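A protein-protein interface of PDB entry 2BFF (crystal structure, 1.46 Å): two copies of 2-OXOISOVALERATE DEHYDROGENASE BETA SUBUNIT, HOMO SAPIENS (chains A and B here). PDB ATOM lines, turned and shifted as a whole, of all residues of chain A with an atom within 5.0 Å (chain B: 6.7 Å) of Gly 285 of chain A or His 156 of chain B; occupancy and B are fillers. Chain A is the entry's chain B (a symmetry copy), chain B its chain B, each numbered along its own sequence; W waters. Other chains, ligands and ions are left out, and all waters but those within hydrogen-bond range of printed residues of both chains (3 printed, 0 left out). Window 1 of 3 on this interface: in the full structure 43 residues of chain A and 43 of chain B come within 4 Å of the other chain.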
ATOM      1  N   SER A 149      -4.281 -37.921  13.432  1.00  0.00           N
ATOM      2  CA  SER A 149      -4.783 -37.171  14.593  1.00  0.00           C
ATOM      3  C   SER A 149      -5.707 -36.051  14.027  1.00  0.00           C
ATOM      4  O   SER A 149      -5.257 -34.909  13.784  1.00  0.00           O
ATOM      5  CB  SER A 149      -3.626 -36.562  15.377  1.00  0.00           C
ATOM      6  OG  SER A 149      -2.643 -36.128  14.480  1.00  0.00           O
ATOM      7  N   ALA A 152      -7.967 -31.175  14.539  1.00  0.00           N
ATOM      8  CA  ALA A 152      -8.152 -29.829  13.937  1.00  0.00           C
ATOM      9  C   ALA A 152      -9.246 -29.756  12.899  1.00  0.00           C
ATOM     10  O   ALA A 152      -9.823 -28.685  12.711  1.00  0.00           O
ATOM     11  CB  ALA A 152      -6.880 -29.336  13.357  1.00  0.00           C
ATOM     12  N   PHE A 153      -9.518 -30.872  12.226  1.00  0.00           N
ATOM     13  CA  PHE A 153     -10.649 -30.835  11.267  1.00  0.00           C
ATOM     14  C   PHE A 153     -11.916 -30.563  12.041  1.00  0.00           C
ATOM     15  O   PHE A 153     -12.812 -29.859  11.558  1.00  0.00           O
ATOM     16  CB  PHE A 153     -10.731 -32.178  10.539  1.00  0.00           C
ATOM     17  CG  PHE A 153      -9.600 -32.453   9.575  1.00  0.00           C
ATOM     18  CD1 PHE A 153      -9.459 -31.647   8.448  1.00  0.00           C
ATOM     19  CD2 PHE A 153      -8.754 -33.554   9.736  1.00  0.00           C
ATOM     20  CE1 PHE A 153      -8.402 -31.918   7.515  1.00  0.00           C
ATOM     21  CE2 PHE A 153      -7.743 -33.809   8.836  1.00  0.00           C
ATOM     22  CZ  PHE A 153      -7.568 -33.030   7.671  1.00  0.00           C
ATOM     23  N   ALA A 281      -0.244 -33.842  14.931  1.00  0.00           N
ATOM     24  CA  ALA A 281      -0.900 -33.484  13.663  1.00  0.00           C
ATOM     25  C   ALA A 281      -0.017 -32.495  12.884  1.00  0.00           C
ATOM     26  O   ALA A 281       0.793 -31.754  13.487  1.00  0.00           O
ATOM     27  CB  ALA A 281      -2.262 -32.874  13.934  1.00  0.00           C
ATOM     28  N   PRO A 282      -0.187 -32.454  11.554  1.00  0.00           N
ATOM     29  CA  PRO A 282       0.543 -31.476  10.771  1.00  0.00           C
ATOM     30  C   PRO A 282       0.374 -30.033  11.261  1.00  0.00           C
ATOM     31  O   PRO A 282      -0.718 -29.616  11.729  1.00  0.00           O
ATOM     32  CB  PRO A 282      -0.129 -31.580   9.383  1.00  0.00           C
ATOM     33  CG  PRO A 282      -0.431 -33.064   9.317  1.00  0.00           C
ATOM     34  CD  PRO A 282      -0.977 -33.385  10.688  1.00  0.00           C
ATOM     35  N   LEU A 283       1.456 -29.287  11.057  1.00  0.00           N
ATOM     36  CA  LEU A 283       1.500 -27.863  11.410  1.00  0.00           C
ATOM     37  C   LEU A 283       0.334 -27.050  10.813  1.00  0.00           C
ATOM     38  O   LEU A 283      -0.368 -26.351  11.559  1.00  0.00           O
ATOM     39  CB  LEU A 283       2.806 -27.270  10.880  1.00  0.00           C
ATOM     40  CG  LEU A 283       2.993 -25.761  11.160  1.00  0.00           C
ATOM     41  CD1 LEU A 283       3.212 -25.476  12.654  1.00  0.00           C
ATOM     42  CD2 LEU A 283       4.133 -25.238  10.306  1.00  0.00           C
ATOM     43  N   THR A 284       0.216 -27.062   9.497  1.00  0.00           N
ATOM     44  CA  THR A 284      -0.636 -26.012   8.837  1.00  0.00           C
ATOM     45  C   THR A 284      -2.089 -26.364   9.137  1.00  0.00           C
ATOM     46  O   THR A 284      -2.587 -27.503   8.859  1.00  0.00           O
ATOM     47  CB  THR A 284      -0.365 -25.982   7.366  1.00  0.00           C
ATOM     48  OG1 THR A 284       0.967 -25.508   7.201  1.00  0.00           O
ATOM     49  CG2 THR A 284      -1.301 -24.994   6.616  1.00  0.00           C
ATOM     50  N   GLY A 285      -2.783 -25.385   9.723  1.00  0.00           N
ATOM     51  CA  GLY A 285      -4.209 -25.635  10.076  1.00  0.00           C
ATOM     52  C   GLY A 285      -4.394 -26.511  11.329  1.00  0.00           C
ATOM     53  O   GLY A 285      -5.518 -26.817  11.739  1.00  0.00           O
ATOM     54  N   GLY A 286      -3.270 -26.929  11.916  1.00  0.00           N
ATOM     55  CA  GLY A 286      -3.344 -27.688  13.178  1.00  0.00           C
ATOM     56  C   GLY A 286      -3.885 -26.873  14.340  1.00  0.00           C
ATOM     57  O   GLY A 286      -3.955 -25.634  14.276  1.00  0.00           O
ATOM     58  N   PHE A 287      -4.267 -27.529  15.423  1.00  0.00           N
ATOM     59  CA  PHE A 287      -4.927 -26.774  16.479  1.00  0.00           C
ATOM     60  C   PHE A 287      -3.972 -25.865  17.226  1.00  0.00           C
ATOM     61  O   PHE A 287      -4.430 -24.885  17.869  1.00  0.00           O
ATOM     62  CB  PHE A 287      -5.710 -27.707  17.455  1.00  0.00           C
ATOM     63  CG  PHE A 287      -6.679 -26.944  18.316  1.00  0.00           C
ATOM     64  CD1 PHE A 287      -7.762 -26.325  17.736  1.00  0.00           C
ATOM     65  CD2 PHE A 287      -6.450 -26.798  19.683  1.00  0.00           C
ATOM     66  CE1 PHE A 287      -8.676 -25.585  18.495  1.00  0.00           C
ATOM     67  CE2 PHE A 287      -7.329 -26.035  20.462  1.00  0.00           C
ATOM     68  CZ  PHE A 287      -8.423 -25.441  19.871  1.00  0.00           C
ATOM     69  N   SER A 289      -2.356 -23.667  15.905  1.00  0.00           N
ATOM     70  CA  SER A 289      -2.566 -22.385  15.267  1.00  0.00           C
ATOM     71  C   SER A 289      -3.617 -21.554  16.029  1.00  0.00           C
ATOM     72  O   SER A 289      -3.467 -20.320  16.183  1.00  0.00           O
ATOM     73  CB  SER A 289      -2.999 -22.628  13.820  1.00  0.00           C
ATOM     74  OG  SER A 289      -3.534 -21.452  13.270  1.00  0.00           O
ATOM     75  N   VAL B 111      -9.775 -36.030   1.334  1.00  0.00           N
ATOM     76  CA  VAL B 111      -8.658 -35.956   2.284  1.00  0.00           C
ATOM     77  C   VAL B 111      -7.890 -37.260   2.318  1.00  0.00           C
ATOM     78  O   VAL B 111      -6.623 -37.243   2.325  1.00  0.00           O
ATOM     79  CB  VAL B 111      -9.202 -35.551   3.655  1.00  0.00           C
ATOM     80  CG1 VAL B 111      -8.204 -35.827   4.783  1.00  0.00           C
ATOM     81  CG2 VAL B 111      -9.685 -34.062   3.642  1.00  0.00           C
ATOM     82  N   LYS B 116      -3.720 -37.628  -0.999  1.00  0.00           N
ATOM     83  CA  LYS B 116      -2.637 -38.553  -0.674  1.00  0.00           C
ATOM     84  C   LYS B 116      -2.228 -39.465  -1.811  1.00  0.00           C
ATOM     85  O   LYS B 116      -1.259 -40.235  -1.668  1.00  0.00           O
ATOM     86  CB  LYS B 116      -3.015 -39.368   0.540  1.00  0.00           C
ATOM     87  CG  LYS B 116      -3.109 -38.502   1.845  1.00  0.00           C
ATOM     88  CD  LYS B 116      -3.882 -39.286   2.962  1.00  0.00           C
ATOM     89  CE  LYS B 116      -3.872 -38.513   4.308  1.00  0.00           C
ATOM     90  NZ  LYS B 116      -4.484 -37.110   4.146  1.00  0.00           N
ATOM     91  N   GLU B 151     -13.188 -23.608   3.771  1.00  0.00           N
ATOM     92  CA  GLU B 151     -11.780 -23.734   3.417  1.00  0.00           C
ATOM     93  C   GLU B 151     -10.847 -24.178   4.553  1.00  0.00           C
ATOM     94  O   GLU B 151      -9.835 -24.849   4.263  1.00  0.00           O
ATOM     95  CB  GLU B 151     -11.272 -22.417   2.802  1.00  0.00           C
ATOM     96  CG  GLU B 151     -11.232 -21.158   3.686  1.00  0.00           C
ATOM     97  CD  GLU B 151     -12.595 -20.431   3.761  1.00  0.00           C
ATOM     98  OE1 GLU B 151     -13.644 -20.964   3.306  1.00  0.00           O
ATOM     99  OE2 GLU B 151     -12.579 -19.259   4.289  1.00  0.00           O
ATOM    100  N   ALA B 152     -11.155 -23.752   5.799  1.00  0.00           N
ATOM    101  CA  ALA B 152     -10.271 -24.206   6.904  1.00  0.00           C
ATOM    102  C   ALA B 152     -10.287 -25.697   7.142  1.00  0.00           C
ATOM    103  O   ALA B 152      -9.295 -26.236   7.630  1.00  0.00           O
ATOM    104  CB  ALA B 152     -10.599 -23.495   8.162  1.00  0.00           C
ATOM    105  N   PHE B 153     -11.402 -26.349   6.819  1.00  0.00           N
ATOM    106  CA  PHE B 153     -11.399 -27.825   6.968  1.00  0.00           C
ATOM    107  C   PHE B 153     -10.362 -28.392   6.027  1.00  0.00           C
ATOM    108  O   PHE B 153      -9.686 -29.375   6.353  1.00  0.00           O
ATOM    109  CB  PHE B 153     -12.791 -28.364   6.635  1.00  0.00           C
ATOM    110  CG  PHE B 153     -13.867 -28.019   7.639  1.00  0.00           C
ATOM    111  CD1 PHE B 153     -13.779 -28.533   8.930  1.00  0.00           C
ATOM    112  CD2 PHE B 153     -14.995 -27.277   7.275  1.00  0.00           C
ATOM    113  CE1 PHE B 153     -14.810 -28.229   9.882  1.00  0.00           C
ATOM    114  CE2 PHE B 153     -15.981 -26.991   8.193  1.00  0.00           C
ATOM    115  CZ  PHE B 153     -15.945 -27.501   9.509  1.00  0.00           C
ATOM    116  N   PHE B 154     -10.264 -27.875   4.822  1.00  0.00           N
ATOM    117  CA  PHE B 154      -9.364 -28.439   3.817  1.00  0.00           C
ATOM    118  C   PHE B 154      -7.922 -27.974   4.008  1.00  0.00           C
ATOM    119  O   PHE B 154      -6.990 -28.637   3.556  1.00  0.00           O
ATOM    120  CB  PHE B 154      -9.875 -28.102   2.408  1.00  0.00           C
ATOM    121  CG  PHE B 154     -11.154 -28.808   2.116  1.00  0.00           C
ATOM    122  CD1 PHE B 154     -11.125 -30.179   1.831  1.00  0.00           C
ATOM    123  CD2 PHE B 154     -12.379 -28.141   2.206  1.00  0.00           C
ATOM    124  CE1 PHE B 154     -12.309 -30.895   1.616  1.00  0.00           C
ATOM    125  CE2 PHE B 154     -13.574 -28.876   1.955  1.00  0.00           C
ATOM    126  CZ  PHE B 154     -13.523 -30.242   1.645  1.00  0.00           C
ATOM    127  N   ALA B 155      -7.751 -26.820   4.694  1.00  0.00           N
ATOM    128  CA  ALA B 155      -6.387 -26.272   4.830  1.00  0.00           C
ATOM    129  C   ALA B 155      -5.487 -27.163   5.655  1.00  0.00           C
ATOM    130  O   ALA B 155      -4.251 -27.031   5.580  1.00  0.00           O
ATOM    131  CB  ALA B 155      -6.473 -24.895   5.469  1.00  0.00           C
ATOM    132  N   HIS B 156      -6.084 -28.056   6.459  1.00  0.00           N
ATOM    133  CA  HIS B 156      -5.279 -28.930   7.343  1.00  0.00           C
ATOM    134  C   HIS B 156      -4.965 -30.246   6.608  1.00  0.00           C
ATOM    135  O   HIS B 156      -4.463 -31.200   7.248  1.00  0.00           O
ATOM    136  CB  HIS B 156      -6.064 -29.170   8.623  1.00  0.00           C
ATOM    137  CG  HIS B 156      -5.325 -29.995   9.643  1.00  0.00           C
ATOM    138  ND1 HIS B 156      -4.060 -29.680  10.095  1.00  0.00           N
ATOM    139  CD2 HIS B 156      -5.702 -31.105  10.330  1.00  0.00           C
ATOM    140  CE1 HIS B 156      -3.667 -30.601  10.991  1.00  0.00           C
ATOM    141  NE2 HIS B 156      -4.655 -31.467  11.160  1.00  0.00           N
ATOM    142  N   CYS B 157      -5.176 -30.310   5.286  1.00  0.00           N
ATOM    143  CA  CYS B 157      -4.872 -31.526   4.494  1.00  0.00           C
ATOM    144  C   CYS B 157      -3.763 -31.346   3.449  1.00  0.00           C
ATOM    145  O   CYS B 157      -4.015 -30.930   2.310  1.00  0.00           O
ATOM    146  CB  CYS B 157      -6.175 -31.988   3.810  1.00  0.00           C
ATOM    147  SG  CYS B 157      -5.911 -33.564   2.992  1.00  0.00           S
ATOM    148  N   PRO B 158      -2.532 -31.681   3.783  1.00  0.00           N
ATOM    149  CA  PRO B 158      -1.460 -31.668   2.781  1.00  0.00           C
ATOM    150  C   PRO B 158      -1.812 -32.481   1.556  1.00  0.00           C
ATOM    151  O   PRO B 158      -2.322 -33.591   1.674  1.00  0.00           O
ATOM    152  CB  PRO B 158      -0.251 -32.288   3.532  1.00  0.00           C
ATOM    153  CG  PRO B 158      -0.562 -31.902   5.033  1.00  0.00           C
ATOM    154  CD  PRO B 158      -2.060 -32.009   5.151  1.00  0.00           C
ATOM    155  N   ILE B 160      -3.701 -31.164  -1.241  1.00  0.00           N
ATOM    156  CA  ILE B 160      -4.703 -30.508  -2.051  1.00  0.00           C
ATOM    157  C   ILE B 160      -4.423 -29.023  -2.061  1.00  0.00           C
ATOM    158  O   ILE B 160      -3.795 -28.481  -1.144  1.00  0.00           O
ATOM    159  CB  ILE B 160      -6.112 -30.732  -1.526  1.00  0.00           C
ATOM    160  CG1 ILE B 160      -6.228 -30.431  -0.034  1.00  0.00           C
ATOM    161  CG2 ILE B 160      -6.542 -32.167  -1.811  1.00  0.00           C
ATOM    162  CD1 ILE B 160      -7.649 -30.455   0.491  1.00  0.00           C
ATOM    163  N   ILE B 258      -4.342 -22.790   0.535  1.00  0.00           N
ATOM    164  CA  ILE B 258      -3.100 -23.600   0.630  1.00  0.00           C
ATOM    165  C   ILE B 258      -2.667 -24.069  -0.721  1.00  0.00           C
ATOM    166  O   ILE B 258      -3.521 -24.391  -1.571  1.00  0.00           O
ATOM    167  CB  ILE B 258      -3.210 -24.824   1.577  1.00  0.00           C
ATOM    168  CG1 ILE B 258      -4.399 -25.713   1.184  1.00  0.00           C
ATOM    169  CG2 ILE B 258      -3.216 -24.361   3.059  1.00  0.00           C
ATOM    170  CD1 ILE B 258      -4.232 -27.134   1.866  1.00  0.00           C
ATOM    171  N   GLY B 285     -10.546 -22.150  14.779  1.00  0.00           N
ATOM    172  CA  GLY B 285     -10.068 -23.110  13.744  1.00  0.00           C
ATOM    173  C   GLY B 285     -10.139 -22.561  12.308  1.00  0.00           C
ATOM    174  O   GLY B 285      -9.791 -23.244  11.340  1.00  0.00           O
ATOM    175  N   GLY B 286     -10.619 -21.321  12.183  1.00  0.00           N
ATOM    176  CA  GLY B 286     -10.631 -20.671  10.860  1.00  0.00           C
ATOM    177  C   GLY B 286      -9.242 -20.404  10.308  1.00  0.00           C
ATOM    178  O   GLY B 286      -8.240 -20.454  11.042  1.00  0.00           O
ATOM    179  N   PHE B 287      -9.140 -20.105   9.023  1.00  0.00           N
ATOM    180  CA  PHE B 287      -7.804 -19.998   8.453  1.00  0.00           C
ATOM    181  C   PHE B 287      -7.073 -18.754   8.919  1.00  0.00           C
ATOM    182  O   PHE B 287      -5.817 -18.716   8.849  1.00  0.00           O
ATOM    183  CB  PHE B 287      -7.830 -20.097   6.896  1.00  0.00           C
ATOM    184  CG  PHE B 287      -6.464 -20.353   6.321  1.00  0.00           C
ATOM    185  CD1 PHE B 287      -5.833 -21.549   6.575  1.00  0.00           C
ATOM    186  CD2 PHE B 287      -5.804 -19.365   5.593  1.00  0.00           C
ATOM    187  CE1 PHE B 287      -4.553 -21.821   6.080  1.00  0.00           C
ATOM    188  CE2 PHE B 287      -4.509 -19.597   5.112  1.00  0.00           C
ATOM    189  CZ  PHE B 287      -3.899 -20.808   5.356  1.00  0.00           C
ATOM    190  N   GLU B 290      -4.202 -19.639  11.216  1.00  0.00           N
ATOM    191  CA  GLU B 290      -2.902 -20.091  10.619  1.00  0.00           C
ATOM    192  C   GLU B 290      -2.082 -18.883  10.183  1.00  0.00           C
ATOM    193  O   GLU B 290      -0.845 -18.798  10.448  1.00  0.00           O
ATOM    194  CB  GLU B 290      -3.115 -21.041   9.466  1.00  0.00           C
ATOM    195  CG  GLU B 290      -1.782 -21.519   8.881  1.00  0.00           C
ATOM    196  CD  GLU B 290      -0.929 -22.301   9.872  1.00  0.00           C
ATOM    197  OE1 GLU B 290      -1.508 -23.087  10.621  1.00  0.00           O
ATOM    198  OE2 GLU B 290       0.271 -22.092   9.861  1.00  0.00           O
HETATM  199  O   HOH W   1      -9.251 -26.004  12.518  1.00  0.00           O
HETATM  200  O   HOH W   2      -5.457 -32.276  13.760  1.00  0.00           O
HETATM  201  O   HOH W   3      -7.416 -25.790   9.585  1.00  0.00           O
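Of the printed residues of chain B, Phe 153 of chain A touches Phe 153 and His 156.
Printed residues of chain B within 4 Å of Leu 283 of chain A: Glu 290 (3.6 Å).
Of chain B, only His 156 and Glu 290 come within 4 Å of Gly 285 of chain A.
Printed residues of chain B within 4 Å of Gly 286 of chain A: His 156 (3.4 Å).
Printed residues of chain A within 4 Å of Phe 153 of chain B: Phe 153 (3.1 Å).
Printed residues of chain A within 4 Å of Ala 155 of chain B: Thr 284 (3.7 Å).
Of the printed residues of chain A, His 156 of chain B touches Ala 152, Phe 153, Ala 281, Pro 282, Thr 284, Gly 285 and Gly 286.
Phe 287 of chain B touches none of the printed residues of chain A.
The nearest printed residue of chain A that does not touch His 156 of chain B is Ser 149 of chain A (4.4 Å).
CD2 of His 156 of chain B touches CB of Ala 152 of chain A, 3.7 Å away.
Phe 153 of chain A touches Phe 153 of chain B.
Phe 153 of chain A touches His 156 of chain B.
Ala 281 of chain A touches His 156 of chain B (CB to NE2, 3.9 Å).
Pro 282 of chain A touches His 156 of chain B (O to CE1, 3.2 Å).
Leu 283 of chain A touches Glu 290 of chain B (O to OE1, 3.6 Å).
Ala 155 of chain B touches Thr 284 of chain A (O to O, 3.7 Å).
Glu 290 of chain B touches Thr 284 of chain A (OE1 to CA, 3.5 Å).
C of Gly 285 of chain A touches ND1 of His 156 of chain B, at 3.4 Å.
Water W2 lies within hydrogen-bond range of O of Ser 149 of chain A (2.6 Å), NE2 of His 156 of chain B (2.8 Å) and N of Ala 152 of chain A (2.8 Å).
Water W3 lies within hydrogen-bond range of O of Ala 152 of chain B and O of Gly 285 of chain A.
Water W1 lies within hydrogen-bond range of O of Ala 152 of chain A and O of Gly 285 of chain B.
Printed residues of chain A that touch a printed residue of chain B: Ala 152, Phe 153, Ala 281, Pro 282, Leu 283, Thr 284, Gly 285, Gly 286 and Ser 289.
Hydrophobic or aromatic side chains of chain A that line the printed part of chain B: Ala 152, Phe 153, Ala 281 and Pro 282.
Among the printed residues, 13 pairs touch across the chains.
Among the printed residues, no Asp or Glu carboxylate lies within 4 Å of a Lys or Arg side-chain nitrogen of the other chain.
A ring nitrogen (ND1) of His 156 of chain B sits at hydrogen-bond distance from the backbone carbonyl oxygen (O) of Thr 284 of chain A, 2.9 Å away.
A ring nitrogen (ND1) of His 156 of chain B is in hydrogen-bond range of the backbone NH of Gly 286 of chain A, at 3.4 Å.
The backbone NH of Gly 285 of chain A lies within hydrogen-bond range of the side-chain carboxylate of Glu 290 of chain B (2.8 Å).
N of Glu 290 of chain B sits at hydrogen-bond distance from OG of Ser 289 of chain A, 2.8 Å away.
N of Ala 281 of chain A sits close to OG of Ser 149 of chain A.
Phe 153 of chain A touches its own counterpart, Phe 153 of chain B.
Positions printed for both chains: 152, 153, 285, 286 and 287.
Of the 13 pairs that touch across the chains among the printed residues, 1 has its exchanged pair printed and touching as well.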
